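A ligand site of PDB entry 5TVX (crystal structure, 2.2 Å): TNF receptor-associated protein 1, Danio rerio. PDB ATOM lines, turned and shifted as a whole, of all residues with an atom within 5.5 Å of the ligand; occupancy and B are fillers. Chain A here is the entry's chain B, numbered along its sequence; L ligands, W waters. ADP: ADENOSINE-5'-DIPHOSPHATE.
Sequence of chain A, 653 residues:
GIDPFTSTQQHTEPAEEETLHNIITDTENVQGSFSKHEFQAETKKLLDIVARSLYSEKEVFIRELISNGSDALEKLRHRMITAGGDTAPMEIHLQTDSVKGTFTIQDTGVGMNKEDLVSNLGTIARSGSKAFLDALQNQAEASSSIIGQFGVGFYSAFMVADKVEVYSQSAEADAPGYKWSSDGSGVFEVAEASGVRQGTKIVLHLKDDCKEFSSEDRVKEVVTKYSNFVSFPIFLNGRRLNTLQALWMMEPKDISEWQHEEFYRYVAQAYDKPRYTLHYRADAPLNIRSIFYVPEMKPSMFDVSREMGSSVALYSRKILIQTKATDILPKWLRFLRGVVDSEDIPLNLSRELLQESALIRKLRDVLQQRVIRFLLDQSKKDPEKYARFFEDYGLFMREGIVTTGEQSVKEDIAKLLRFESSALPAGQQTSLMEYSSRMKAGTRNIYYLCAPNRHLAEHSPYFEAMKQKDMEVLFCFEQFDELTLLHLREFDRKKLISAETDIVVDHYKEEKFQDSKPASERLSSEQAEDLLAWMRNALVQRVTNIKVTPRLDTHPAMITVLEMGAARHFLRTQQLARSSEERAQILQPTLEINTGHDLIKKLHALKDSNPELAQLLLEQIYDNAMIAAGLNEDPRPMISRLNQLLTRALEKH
The side-chain hydroxyl of Ser 127 sits at hydrogen-bond distance from an oxygen (O3B) of the ligand, 2.6 Å away. O1B of the ligand sits at hydrogen-bond distance from N of Gln 149. The backbone NH (N) of Phe 154 is in hydrogen-bond range of an oxygen (O1A) of the ligand (2.8 Å). The backbone NH of Gly 151 is in hydrogen-bond range of an oxygen (O1B) of the ligand, 2.8 Å away. The side-chain carboxylate of Asp 107 is in hydrogen-bond range of a nitrogen (N6) of the ligand. O2B of the ligand lies close to OD1 of Asn 68. ND2 of Asn 120 is in hydrogen-bond range of O2' of the ligand (2.9 Å). N of Gly 128 lies within hydrogen-bond range of O3' of the ligand. O1B of the ligand sits at hydrogen-bond distance from N of Phe 150 (3.0 Å). The backbone NH (N) of Ser 129 lies within hydrogen-bond range of an oxygen (O3') of the ligand. OG of Ser 129 lies within hydrogen-bond range of O3' of the ligand (3.3 Å). An oxygen (O2A) of the ligand sits at hydrogen-bond distance from the backbone NH (N) of Val 152 (3.2 Å). N1 of the ligand sits at hydrogen-bond distance from OG1 of Thr 200 (3.3 Å). The backbone NH (N) of Gly 153 lies within hydrogen-bond range of an oxygen (O1A) of the ligand, 3.3 Å away. The side-chain amino group of Lys 75 sits at hydrogen-bond distance from an oxygen (O2') of the ligand, at 3.4 Å.
The backbone NH of Lys 130 lies within hydrogen-bond range of the side-chain hydroxyl of Ser 127 (3.4 Å). The backbone NH of Asp 107 is in hydrogen-bond range of the backbone carbonyl oxygen of Thr 200 (3.0 Å). The side-chain hydroxyl of Ser 129 is in hydrogen-bond range of the side-chain amino group of Lys 75 (2.7 Å). The side-chain hydroxyl (OG1) of Thr 200 sits at hydrogen-bond distance from the side-chain hydroxyl (OG) of Ser 168. O of Ala 72 sits at hydrogen-bond distance from N of Val 110. The side-chain hydroxyl (OG) of Ser 168 lies within hydrogen-bond range of the backbone NH (N) of Met 112, 2.8 Å away. The backbone NH (N) of Gly 148 sits at hydrogen-bond distance from the side-chain carboxylate (OD2) of Asp 71, at 2.8 Å.
The side-chain sulfur (SD) of Met 112 sits close to a nitrogen (N3) of the ligand, at 3.7 Å. Ala 72 touches the ligand (CB to N1, 3.4 Å). Gly 111 touches the ligand (O to C2, 3.9 Å). Arg 126 touches the ligand. CA of Gly 148 touches O1B of the ligand (3.5 Å). Hydrophobic or aromatic side chains within 4 Å of the ligand: Ala 72, Met 112 and Phe 154. Within 4 Å of the ligand: Asn 68, Ala 72, Lys 75, Asp 107, Gly 111, Met 112, Asn 120, Arg 126, Ser 127, Gly 128, Ser 129, Gly 148, Gln 149, Phe 150, Gly 151, Val 152, Gly 153, Phe 154 and Thr 200.
Water W9 lies within hydrogen-bond range of ND2 of Asn 68 (2.7 Å) and N7 of the ligand (2.7 Å). Water W7 lies within hydrogen-bond range of the side-chain hydroxyl of Thr 200, the side-chain carboxylate of Asp 107, the backbone NH of Gly 111 and a nitrogen (N1) of the ligand. Water W6 lies within hydrogen-bond range of OE1 of Glu 64 (2.6 Å), OD1 of Asn 68 (3.1 Å) and O2B of the ligand (3.3 Å). Water W3 lies within hydrogen-bond range of OG of Ser 129 (2.7 Å), OD2 of Asp 71 (2.9 Å), OD1 of Asn 68 (3.3 Å) and O2B of the ligand (3.3 Å). Water W1 bridges O of Leu 65 and N6 of the ligand. Water W2 lies within hydrogen-bond range of OD2 of Asp 71 (2.7 Å), OD1 of Asn 68 (2.9 Å), N of Gly 148 (3.3 Å) and O2B of the ligand (3.4 Å).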
ATOM      1  N   GLU A  64       6.557  -5.769  -0.857  1.00  0.00           N
ATOM      2  CA  GLU A  64       6.454  -4.709   0.153  1.00  0.00           C
ATOM      3  C   GLU A  64       5.838  -3.439  -0.435  1.00  0.00           C
ATOM      4  O   GLU A  64       4.963  -2.823   0.182  1.00  0.00           O
ATOM      5  CB  GLU A  64       7.826  -4.395   0.749  1.00  0.00           C
ATOM      6  CG  GLU A  64       8.430  -5.519   1.526  1.00  0.00           C
ATOM      7  CD  GLU A  64       7.504  -5.984   2.639  1.00  0.00           C
ATOM      8  OE1 GLU A  64       7.025  -5.133   3.417  1.00  0.00           O
ATOM      9  OE2 GLU A  64       7.266  -7.197   2.731  1.00  0.00           O
ATOM     10  N   LEU A  65       6.313  -3.006  -1.604  1.00  0.00           N
ATOM     11  CA  LEU A  65       5.778  -1.771  -2.171  1.00  0.00           C
ATOM     12  C   LEU A  65       4.322  -1.960  -2.631  1.00  0.00           C
ATOM     13  O   LEU A  65       3.512  -1.036  -2.475  1.00  0.00           O
ATOM     14  CB  LEU A  65       6.646  -1.278  -3.324  1.00  0.00           C
ATOM     15  CG  LEU A  65       8.140  -1.082  -3.002  1.00  0.00           C
ATOM     16  CD1 LEU A  65       8.935  -0.487  -4.206  1.00  0.00           C
ATOM     17  CD2 LEU A  65       8.280  -0.212  -1.805  1.00  0.00           C
ATOM     18  N   ASN A  68       2.051  -1.709   0.457  1.00  0.00           N
ATOM     19  CA  ASN A  68       1.881  -0.304   0.823  1.00  0.00           C
ATOM     20  C   ASN A  68       0.881   0.380  -0.105  1.00  0.00           C
ATOM     21  O   ASN A  68       0.107   1.245   0.339  1.00  0.00           O
ATOM     22  CB  ASN A  68       3.215   0.435   0.782  1.00  0.00           C
ATOM     23  CG  ASN A  68       4.105   0.088   1.957  1.00  0.00           C
ATOM     24  OD1 ASN A  68       3.658  -0.598   2.867  1.00  0.00           O
ATOM     25  ND2 ASN A  68       5.368   0.545   1.948  1.00  0.00           N
ATOM     26  N   GLY A  69       0.900   0.028  -1.389  1.00  0.00           N
ATOM     27  CA  GLY A  69      -0.052   0.620  -2.320  1.00  0.00           C
ATOM     28  C   GLY A  69      -1.457   0.175  -2.019  1.00  0.00           C
ATOM     29  O   GLY A  69      -2.390   0.983  -2.046  1.00  0.00           O
ATOM     30  N   ASP A  71      -2.578  -0.744   0.981  1.00  0.00           N
ATOM     31  CA  ASP A  71      -3.001  -0.066   2.209  1.00  0.00           C
ATOM     32  C   ASP A  71      -3.408   1.374   1.940  1.00  0.00           C
ATOM     33  O   ASP A  71      -4.411   1.851   2.485  1.00  0.00           O
ATOM     34  CB  ASP A  71      -1.888  -0.121   3.256  1.00  0.00           C
ATOM     35  CG  ASP A  71      -1.614  -1.538   3.762  1.00  0.00           C
ATOM     36  OD1 ASP A  71      -2.416  -2.469   3.506  1.00  0.00           O
ATOM     37  OD2 ASP A  71      -0.576  -1.719   4.426  1.00  0.00           O
ATOM     38  N   ALA A  72      -2.664   2.080   1.094  1.00  0.00           N
ATOM     39  CA  ALA A  72      -3.042   3.438   0.726  1.00  0.00           C
ATOM     40  C   ALA A  72      -4.410   3.461   0.031  1.00  0.00           C
ATOM     41  O   ALA A  72      -5.211   4.368   0.266  1.00  0.00           O
ATOM     42  CB  ALA A  72      -1.968   4.054  -0.176  1.00  0.00           C
ATOM     43  N   LYS A  75      -7.083   2.949   2.696  1.00  0.00           N
ATOM     44  CA  LYS A  75      -7.358   4.174   3.439  1.00  0.00           C
ATOM     45  C   LYS A  75      -8.211   5.132   2.622  1.00  0.00           C
ATOM     46  O   LYS A  75      -9.024   5.880   3.196  1.00  0.00           O
ATOM     47  CB  LYS A  75      -6.055   4.829   3.866  1.00  0.00           C
ATOM     48  CG  LYS A  75      -5.220   3.969   4.803  1.00  0.00           C
ATOM     49  CD  LYS A  75      -3.849   4.571   5.033  1.00  0.00           C
ATOM     50  CE  LYS A  75      -2.972   3.627   5.835  1.00  0.00           C
ATOM     51  NZ  LYS A  75      -1.633   4.247   6.129  1.00  0.00           N
ATOM     52  N   ASP A 107       0.375   4.057  -6.978  1.00  0.00           N
ATOM     53  CA  ASP A 107      -0.987   3.812  -6.555  1.00  0.00           C
ATOM     54  C   ASP A 107      -1.769   5.119  -6.579  1.00  0.00           C
ATOM     55  O   ASP A 107      -1.185   6.214  -6.533  1.00  0.00           O
ATOM     56  CB  ASP A 107      -1.069   3.201  -5.157  1.00  0.00           C
ATOM     57  CG  ASP A 107      -0.559   4.142  -4.100  1.00  0.00           C
ATOM     58  OD1 ASP A 107       0.614   3.971  -3.681  1.00  0.00           O
ATOM     59  OD2 ASP A 107      -1.311   5.055  -3.687  1.00  0.00           O
ATOM     60  N   VAL A 110      -4.423   7.340  -0.785  1.00  0.00           N
ATOM     61  CA  VAL A 110      -4.537   8.592  -0.015  1.00  0.00           C
ATOM     62  C   VAL A 110      -3.331   9.503  -0.154  1.00  0.00           C
ATOM     63  O   VAL A 110      -3.405  10.669   0.231  1.00  0.00           O
ATOM     64  CB  VAL A 110      -4.769   8.317   1.484  1.00  0.00           C
ATOM     65  CG1 VAL A 110      -6.136   7.736   1.706  1.00  0.00           C
ATOM     66  CG2 VAL A 110      -3.685   7.393   2.041  1.00  0.00           C
ATOM     67  N   GLY A 111      -2.204   9.002  -0.630  1.00  0.00           N
ATOM     68  CA  GLY A 111      -1.009   9.834  -0.677  1.00  0.00           C
ATOM     69  C   GLY A 111      -0.535  10.228   0.708  1.00  0.00           C
ATOM     70  O   GLY A 111      -1.011   9.741   1.741  1.00  0.00           O
ATOM     71  N   MET A 112       0.436  11.127   0.724  1.00  0.00           N
ATOM     72  CA  MET A 112       1.035  11.638   1.943  1.00  0.00           C
ATOM     73  C   MET A 112       1.323  13.124   1.768  1.00  0.00           C
ATOM     74  O   MET A 112       1.709  13.563   0.666  1.00  0.00           O
ATOM     75  CB  MET A 112       2.347  10.911   2.287  1.00  0.00           C
ATOM     76  CG  MET A 112       2.241   9.437   2.657  1.00  0.00           C
ATOM     77  SD  MET A 112       3.902   8.673   2.842  1.00  0.00           S
ATOM     78  CE  MET A 112       4.208   8.181   1.148  1.00  0.00           C
ATOM     79  N   ASN A 120       6.693   9.185   8.126  1.00  0.00           N
ATOM     80  CA  ASN A 120       6.480   7.769   7.859  1.00  0.00           C
ATOM     81  C   ASN A 120       7.663   7.159   7.121  1.00  0.00           C
ATOM     82  O   ASN A 120       8.116   6.068   7.476  1.00  0.00           O
ATOM     83  CB  ASN A 120       5.188   7.587   7.069  1.00  0.00           C
ATOM     84  CG  ASN A 120       3.943   7.774   7.930  1.00  0.00           C
ATOM     85  OD1 ASN A 120       4.026   7.998   9.139  1.00  0.00           O
ATOM     86  ND2 ASN A 120       2.779   7.694   7.293  1.00  0.00           N
ATOM     87  N   LEU A 121       8.158   7.850   6.089  1.00  0.00           N
ATOM     88  CA  LEU A 121       9.326   7.338   5.369  1.00  0.00           C
ATOM     89  C   LEU A 121      10.622   7.621   6.114  1.00  0.00           C
ATOM     90  O   LEU A 121      11.576   6.839   6.018  1.00  0.00           O
ATOM     91  CB  LEU A 121       9.382   7.923   3.945  1.00  0.00           C
ATOM     92  CG  LEU A 121       8.165   7.673   3.038  1.00  0.00           C
ATOM     93  CD1 LEU A 121       8.421   8.149   1.598  1.00  0.00           C
ATOM     94  CD2 LEU A 121       7.811   6.209   3.052  1.00  0.00           C
ATOM     95  N   ARG A 126       8.346   3.356  12.103  1.00  0.00           N
ATOM     96  CA  ARG A 126       7.119   4.135  12.158  1.00  0.00           C
ATOM     97  C   ARG A 126       6.160   3.655  11.080  1.00  0.00           C
ATOM     98  O   ARG A 126       6.529   3.590   9.901  1.00  0.00           O
ATOM     99  CB  ARG A 126       7.396   5.634  11.969  1.00  0.00           C
ATOM    100  CG  ARG A 126       6.135   6.494  12.027  1.00  0.00           C
ATOM    101  CD  ARG A 126       6.446   7.851  12.636  1.00  0.00           C
ATOM    102  NE  ARG A 126       6.801   7.731  14.042  1.00  0.00           N
ATOM    103  CZ  ARG A 126       7.368   8.700  14.763  1.00  0.00           C
ATOM    104  NH1 ARG A 126       7.664   9.857  14.193  1.00  0.00           N
ATOM    105  NH2 ARG A 126       7.654   8.491  16.051  1.00  0.00           N
ATOM    106  N   SER A 127       4.940   3.321  11.495  1.00  0.00           N
ATOM    107  CA  SER A 127       3.894   2.846  10.593  1.00  0.00           C
ATOM    108  C   SER A 127       2.666   3.716  10.754  1.00  0.00           C
ATOM    109  O   SER A 127       1.962   3.619  11.768  1.00  0.00           O
ATOM    110  CB  SER A 127       3.539   1.390  10.872  1.00  0.00           C
ATOM    111  OG  SER A 127       2.599   0.970   9.905  1.00  0.00           O
ATOM    112  N   GLY A 128       2.398   4.568   9.768  1.00  0.00           N
ATOM    113  CA  GLY A 128       1.125   5.262   9.738  1.00  0.00           C
ATOM    114  C   GLY A 128      -0.038   4.295   9.748  1.00  0.00           C
ATOM    115  O   GLY A 128      -1.011   4.478  10.487  1.00  0.00           O
ATOM    116  N   SER A 129       0.065   3.233   8.950  1.00  0.00           N
ATOM    117  CA  SER A 129      -0.966   2.210   8.840  1.00  0.00           C
ATOM    118  C   SER A 129      -1.201   1.435  10.142  1.00  0.00           C
ATOM    119  O   SER A 129      -2.083   0.571  10.156  1.00  0.00           O
ATOM    120  CB  SER A 129      -0.612   1.226   7.713  1.00  0.00           C
ATOM    121  OG  SER A 129      -0.379   1.903   6.493  1.00  0.00           O
ATOM    122  N   LYS A 130      -0.454   1.702  11.205  1.00  0.00           N
ATOM    123  CA  LYS A 130      -0.777   1.150  12.515  1.00  0.00           C
ATOM    124  C   LYS A 130      -1.493   2.159  13.408  1.00  0.00           C
ATOM    125  O   LYS A 130      -2.356   1.769  14.203  1.00  0.00           O
ATOM    126  CB  LYS A 130       0.487   0.634  13.224  1.00  0.00           C
ATOM    127  CG  LYS A 130       0.223  -0.577  14.110  1.00  0.00           C
ATOM    128  CD  LYS A 130      -0.320  -1.761  13.291  1.00  0.00           C
ATOM    129  CE  LYS A 130      -0.873  -2.880  14.167  1.00  0.00           C
ATOM    130  NZ  LYS A 130      -2.254  -2.607  14.706  1.00  0.00           N
ATOM    131  N   GLY A 148       0.244  -3.342   6.559  1.00  0.00           N
ATOM    132  CA  GLY A 148       1.384  -2.716   7.222  1.00  0.00           C
ATOM    133  C   GLY A 148       1.280  -2.717   8.734  1.00  0.00           C
ATOM    134  O   GLY A 148       0.188  -2.704   9.300  1.00  0.00           O
ATOM    135  N   GLN A 149       2.441  -2.721   9.382  1.00  0.00           N
ATOM    136  CA  GLN A 149       2.500  -2.803  10.847  1.00  0.00           C
ATOM    137  C   GLN A 149       3.900  -2.513  11.407  1.00  0.00           C
ATOM    138  O   GLN A 149       4.028  -1.831  12.424  1.00  0.00           O
ATOM    139  CB  GLN A 149       2.043  -4.188  11.276  1.00  0.00           C
ATOM    140  CG  GLN A 149       2.087  -4.437  12.756  1.00  0.00           C
ATOM    141  CD  GLN A 149       2.263  -5.899  13.075  1.00  0.00           C
ATOM    142  OE1 GLN A 149       2.183  -6.745  12.164  1.00  0.00           O
ATOM    143  NE2 GLN A 149       2.505  -6.217  14.348  1.00  0.00           N
ATOM    144  N   PHE A 150       4.940  -3.001  10.720  1.00  0.00           N
ATOM    145  CA  PHE A 150       6.307  -2.953  11.217  1.00  0.00           C
ATOM    146  C   PHE A 150       7.033  -1.647  10.929  1.00  0.00           C
ATOM    147  O   PHE A 150       7.976  -1.309  11.653  1.00  0.00           O
ATOM    148  CB  PHE A 150       7.099  -4.113  10.614  1.00  0.00           C
ATOM    149  CG  PHE A 150       6.714  -5.463  11.173  1.00  0.00           C
ATOM    150  CD1 PHE A 150       6.614  -5.659  12.543  1.00  0.00           C
ATOM    151  CD2 PHE A 150       6.440  -6.533  10.307  1.00  0.00           C
ATOM    152  CE1 PHE A 150       6.260  -6.899  13.063  1.00  0.00           C
ATOM    153  CE2 PHE A 150       6.089  -7.770  10.814  1.00  0.00           C
ATOM    154  CZ  PHE A 150       5.980  -7.958  12.191  1.00  0.00           C
ATOM    155  N   GLY A 151       6.662  -0.908   9.895  1.00  0.00           N
ATOM    156  CA  GLY A 151       7.342   0.345   9.617  1.00  0.00           C
ATOM    157  C   GLY A 151       8.685   0.232   8.949  1.00  0.00           C
ATOM    158  O   GLY A 151       9.550   1.091   9.158  1.00  0.00           O
ATOM    159  N   VAL A 152       8.915  -0.822   8.160  1.00  0.00           N
ATOM    160  CA  VAL A 152      10.235  -1.100   7.602  1.00  0.00           C
ATOM    161  C   VAL A 152      10.138  -1.587   6.175  1.00  0.00           C
ATOM    162  O   VAL A 152      11.148  -1.619   5.452  1.00  0.00           O
ATOM    163  CB  VAL A 152      11.003  -2.144   8.438  1.00  0.00           C
ATOM    164  CG1 VAL A 152      11.109  -1.712   9.884  1.00  0.00           C
ATOM    165  CG2 VAL A 152      10.344  -3.513   8.279  1.00  0.00           C
ATOM    166  N   GLY A 153       8.949  -2.016   5.749  1.00  0.00           N
ATOM    167  CA  GLY A 153       8.815  -2.648   4.433  1.00  0.00           C
ATOM    168  C   GLY A 153       9.339  -1.764   3.306  1.00  0.00           C
ATOM    169  O   GLY A 153       9.996  -2.248   2.385  1.00  0.00           O
ATOM    170  N   PHE A 154       9.056  -0.464   3.382  1.00  0.00           N
ATOM    171  CA  PHE A 154       9.469   0.455   2.331  1.00  0.00           C
ATOM    172  C   PHE A 154      10.984   0.406   2.102  1.00  0.00           C
ATOM    173  O   PHE A 154      11.444   0.457   0.955  1.00  0.00           O
ATOM    174  CB  PHE A 154       8.990   1.868   2.696  1.00  0.00           C
ATOM    175  CG  PHE A 154       9.620   2.996   1.879  1.00  0.00           C
ATOM    176  CD1 PHE A 154      10.673   3.741   2.404  1.00  0.00           C
ATOM    177  CD2 PHE A 154       9.139   3.321   0.616  1.00  0.00           C
ATOM    178  CE1 PHE A 154      11.232   4.775   1.695  1.00  0.00           C
ATOM    179  CE2 PHE A 154       9.701   4.358  -0.107  1.00  0.00           C
ATOM    180  CZ  PHE A 154      10.751   5.081   0.429  1.00  0.00           C
ATOM    181  N   TYR A 155      11.774   0.273   3.179  1.00  0.00           N
ATOM    182  CA  TYR A 155      13.237   0.342   3.023  1.00  0.00           C
ATOM    183  C   TYR A 155      13.784  -0.817   2.210  1.00  0.00           C
ATOM    184  O   TYR A 155      14.926  -0.749   1.749  1.00  0.00           O
ATOM    185  CB  TYR A 155      13.947   0.442   4.405  1.00  0.00           C
ATOM    186  CG  TYR A 155      13.312   1.512   5.252  1.00  0.00           C
ATOM    187  CD1 TYR A 155      13.406   2.852   4.889  1.00  0.00           C
ATOM    188  CD2 TYR A 155      12.527   1.181   6.365  1.00  0.00           C
ATOM    189  CE1 TYR A 155      12.775   3.844   5.618  1.00  0.00           C
ATOM    190  CE2 TYR A 155      11.873   2.173   7.097  1.00  0.00           C
ATOM    191  CZ  TYR A 155      12.000   3.507   6.710  1.00  0.00           C
ATOM    192  OH  TYR A 155      11.385   4.491   7.425  1.00  0.00           O
ATOM    193  N   SER A 168       4.318  12.242  -4.031  1.00  0.00           N
ATOM    194  CA  SER A 168       3.098  11.917  -3.314  1.00  0.00           C
ATOM    195  C   SER A 168       2.185  13.137  -3.262  1.00  0.00           C
ATOM    196  O   SER A 168       2.661  14.280  -3.202  1.00  0.00           O
ATOM    197  CB  SER A 168       3.390  11.408  -1.903  1.00  0.00           C
ATOM    198  OG  SER A 168       2.251  10.757  -1.385  1.00  0.00           O
ATOM    199  N   THR A 200       0.590   8.064  -4.946  1.00  0.00           N
ATOM    200  CA  THR A 200       2.021   8.035  -4.673  1.00  0.00           C
ATOM    201  C   THR A 200       2.731   7.284  -5.786  1.00  0.00           C
ATOM    202  O   THR A 200       2.269   6.226  -6.213  1.00  0.00           O
ATOM    203  CB  THR A 200       2.288   7.382  -3.310  1.00  0.00           C
ATOM    204  OG1 THR A 200       1.598   8.099  -2.281  1.00  0.00           O
ATOM    205  CG2 THR A 200       3.762   7.355  -2.992  1.00  0.00           C
ATOM    206  N   ILE A 202       6.626   5.834  -6.851  1.00  0.00           N
ATOM    207  CA  ILE A 202       7.956   5.509  -6.326  1.00  0.00           C
ATOM    208  C   ILE A 202       8.813   4.959  -7.467  1.00  0.00           C
ATOM    209  O   ILE A 202       8.463   3.939  -8.080  1.00  0.00           O
ATOM    210  CB  ILE A 202       7.883   4.500  -5.175  1.00  0.00           C
ATOM    211  CG1 ILE A 202       6.905   4.972  -4.101  1.00  0.00           C
ATOM    212  CG2 ILE A 202       9.263   4.276  -4.592  1.00  0.00           C
ATOM    213  CD1 ILE A 202       6.815   4.048  -2.921  1.00  0.00           C
ATOM    214  N   ARG A 351       8.412 -11.916   7.110  1.00  0.00           N
ATOM    215  CA  ARG A 351       7.234 -12.533   6.501  1.00  0.00           C
ATOM    216  C   ARG A 351       7.616 -13.770   5.715  1.00  0.00           C
ATOM    217  O   ARG A 351       7.071 -14.035   4.644  1.00  0.00           O
ATOM    218  CB  ARG A 351       6.459 -11.549   5.607  1.00  0.00           C
ATOM    219  CG  ARG A 351       5.875 -10.337   6.308  1.00  0.00           C
ATOM    220  CD  ARG A 351       5.426  -9.293   5.278  1.00  0.00           C
ATOM    221  NE  ARG A 351       5.111  -8.010   5.887  1.00  0.00           N
ATOM    222  CZ  ARG A 351       3.959  -7.743   6.509  1.00  0.00           C
ATOM    223  NH1 ARG A 351       3.039  -8.696   6.608  1.00  0.00           N
ATOM    224  NH2 ARG A 351       3.756  -6.544   7.032  1.00  0.00           N
HETATM  225  PB  ADP L   1       4.457  -0.425   7.061  1.00  0.00           P
HETATM  226  O1B ADP L   1       4.578  -1.504   8.107  1.00  0.00           O
HETATM  227  O2B ADP L   1       4.239  -0.958   5.662  1.00  0.00           O
HETATM  228  O3B ADP L   1       3.589   0.694   7.510  1.00  0.00           O
HETATM  229  PA  ADP L   1       6.636   1.058   5.883  1.00  0.00           P
HETATM  230  O1A ADP L   1       6.670   0.162   4.667  1.00  0.00           O
HETATM  231  O2A ADP L   1       7.914   1.672   6.407  1.00  0.00           O
HETATM  232  O3A ADP L   1       5.909   0.292   7.079  1.00  0.00           O
HETATM  233  O5' ADP L   1       5.631   2.286   5.592  1.00  0.00           O
HETATM  234  C5' ADP L   1       5.673   3.477   6.361  1.00  0.00           C
HETATM  235  C4' ADP L   1       4.379   4.276   6.218  1.00  0.00           C
HETATM  236  O4' ADP L   1       4.421   5.195   5.109  1.00  0.00           O
HETATM  237  C3' ADP L   1       3.125   3.443   6.020  1.00  0.00           C
HETATM  238  O3' ADP L   1       2.625   3.009   7.294  1.00  0.00           O
HETATM  239  C2' ADP L   1       2.188   4.448   5.373  1.00  0.00           C
HETATM  240  O2' ADP L   1       1.581   5.211   6.425  1.00  0.00           O
HETATM  241  C1' ADP L   1       3.118   5.359   4.571  1.00  0.00           C
HETATM  242  N9  ADP L   1       3.154   4.890   3.164  1.00  0.00           N
HETATM  243  C8  ADP L   1       4.032   4.017   2.656  1.00  0.00           C
HETATM  244  N7  ADP L   1       3.816   3.793   1.343  1.00  0.00           N
HETATM  245  C5  ADP L   1       2.756   4.552   0.998  1.00  0.00           C
HETATM  246  C6  ADP L   1       2.004   4.801  -0.246  1.00  0.00           C
HETATM  247  N6  ADP L   1       2.302   4.169  -1.399  1.00  0.00           N
HETATM  248  N1  ADP L   1       0.971   5.670  -0.177  1.00  0.00           N
HETATM  249  C2  ADP L   1       0.646   6.303   0.972  1.00  0.00           C
HETATM  250  N3  ADP L   1       1.286   6.133   2.125  1.00  0.00           N
HETATM  251  C4  ADP L   1       2.331   5.276   2.199  1.00  0.00           C
HETATM  252  O   HOH W   1       4.030   1.520  -2.589  1.00  0.00           O
HETATM  253  O   HOH W   2       1.899  -2.690   3.833  1.00  0.00           O
HETATM  254  O   HOH W   3       1.311   0.422   4.927  1.00  0.00           O
HETATM  255  O   HOH W   4       0.220   6.998   4.729  1.00  0.00           O
HETATM  256  O   HOH W   5       8.753   3.608   8.199  1.00  0.00           O
HETATM  257  O   HOH W   6       5.714  -2.883   3.463  1.00  0.00           O
HETATM  258  O   HOH W   7      -0.681   7.115  -1.957  1.00  0.00           O
HETATM  259  O   HOH W   8       6.504  -2.999   7.018  1.00  0.00           O
HETATM  260  O   HOH W   9       5.695   2.374   0.028  1.00  0.00           O
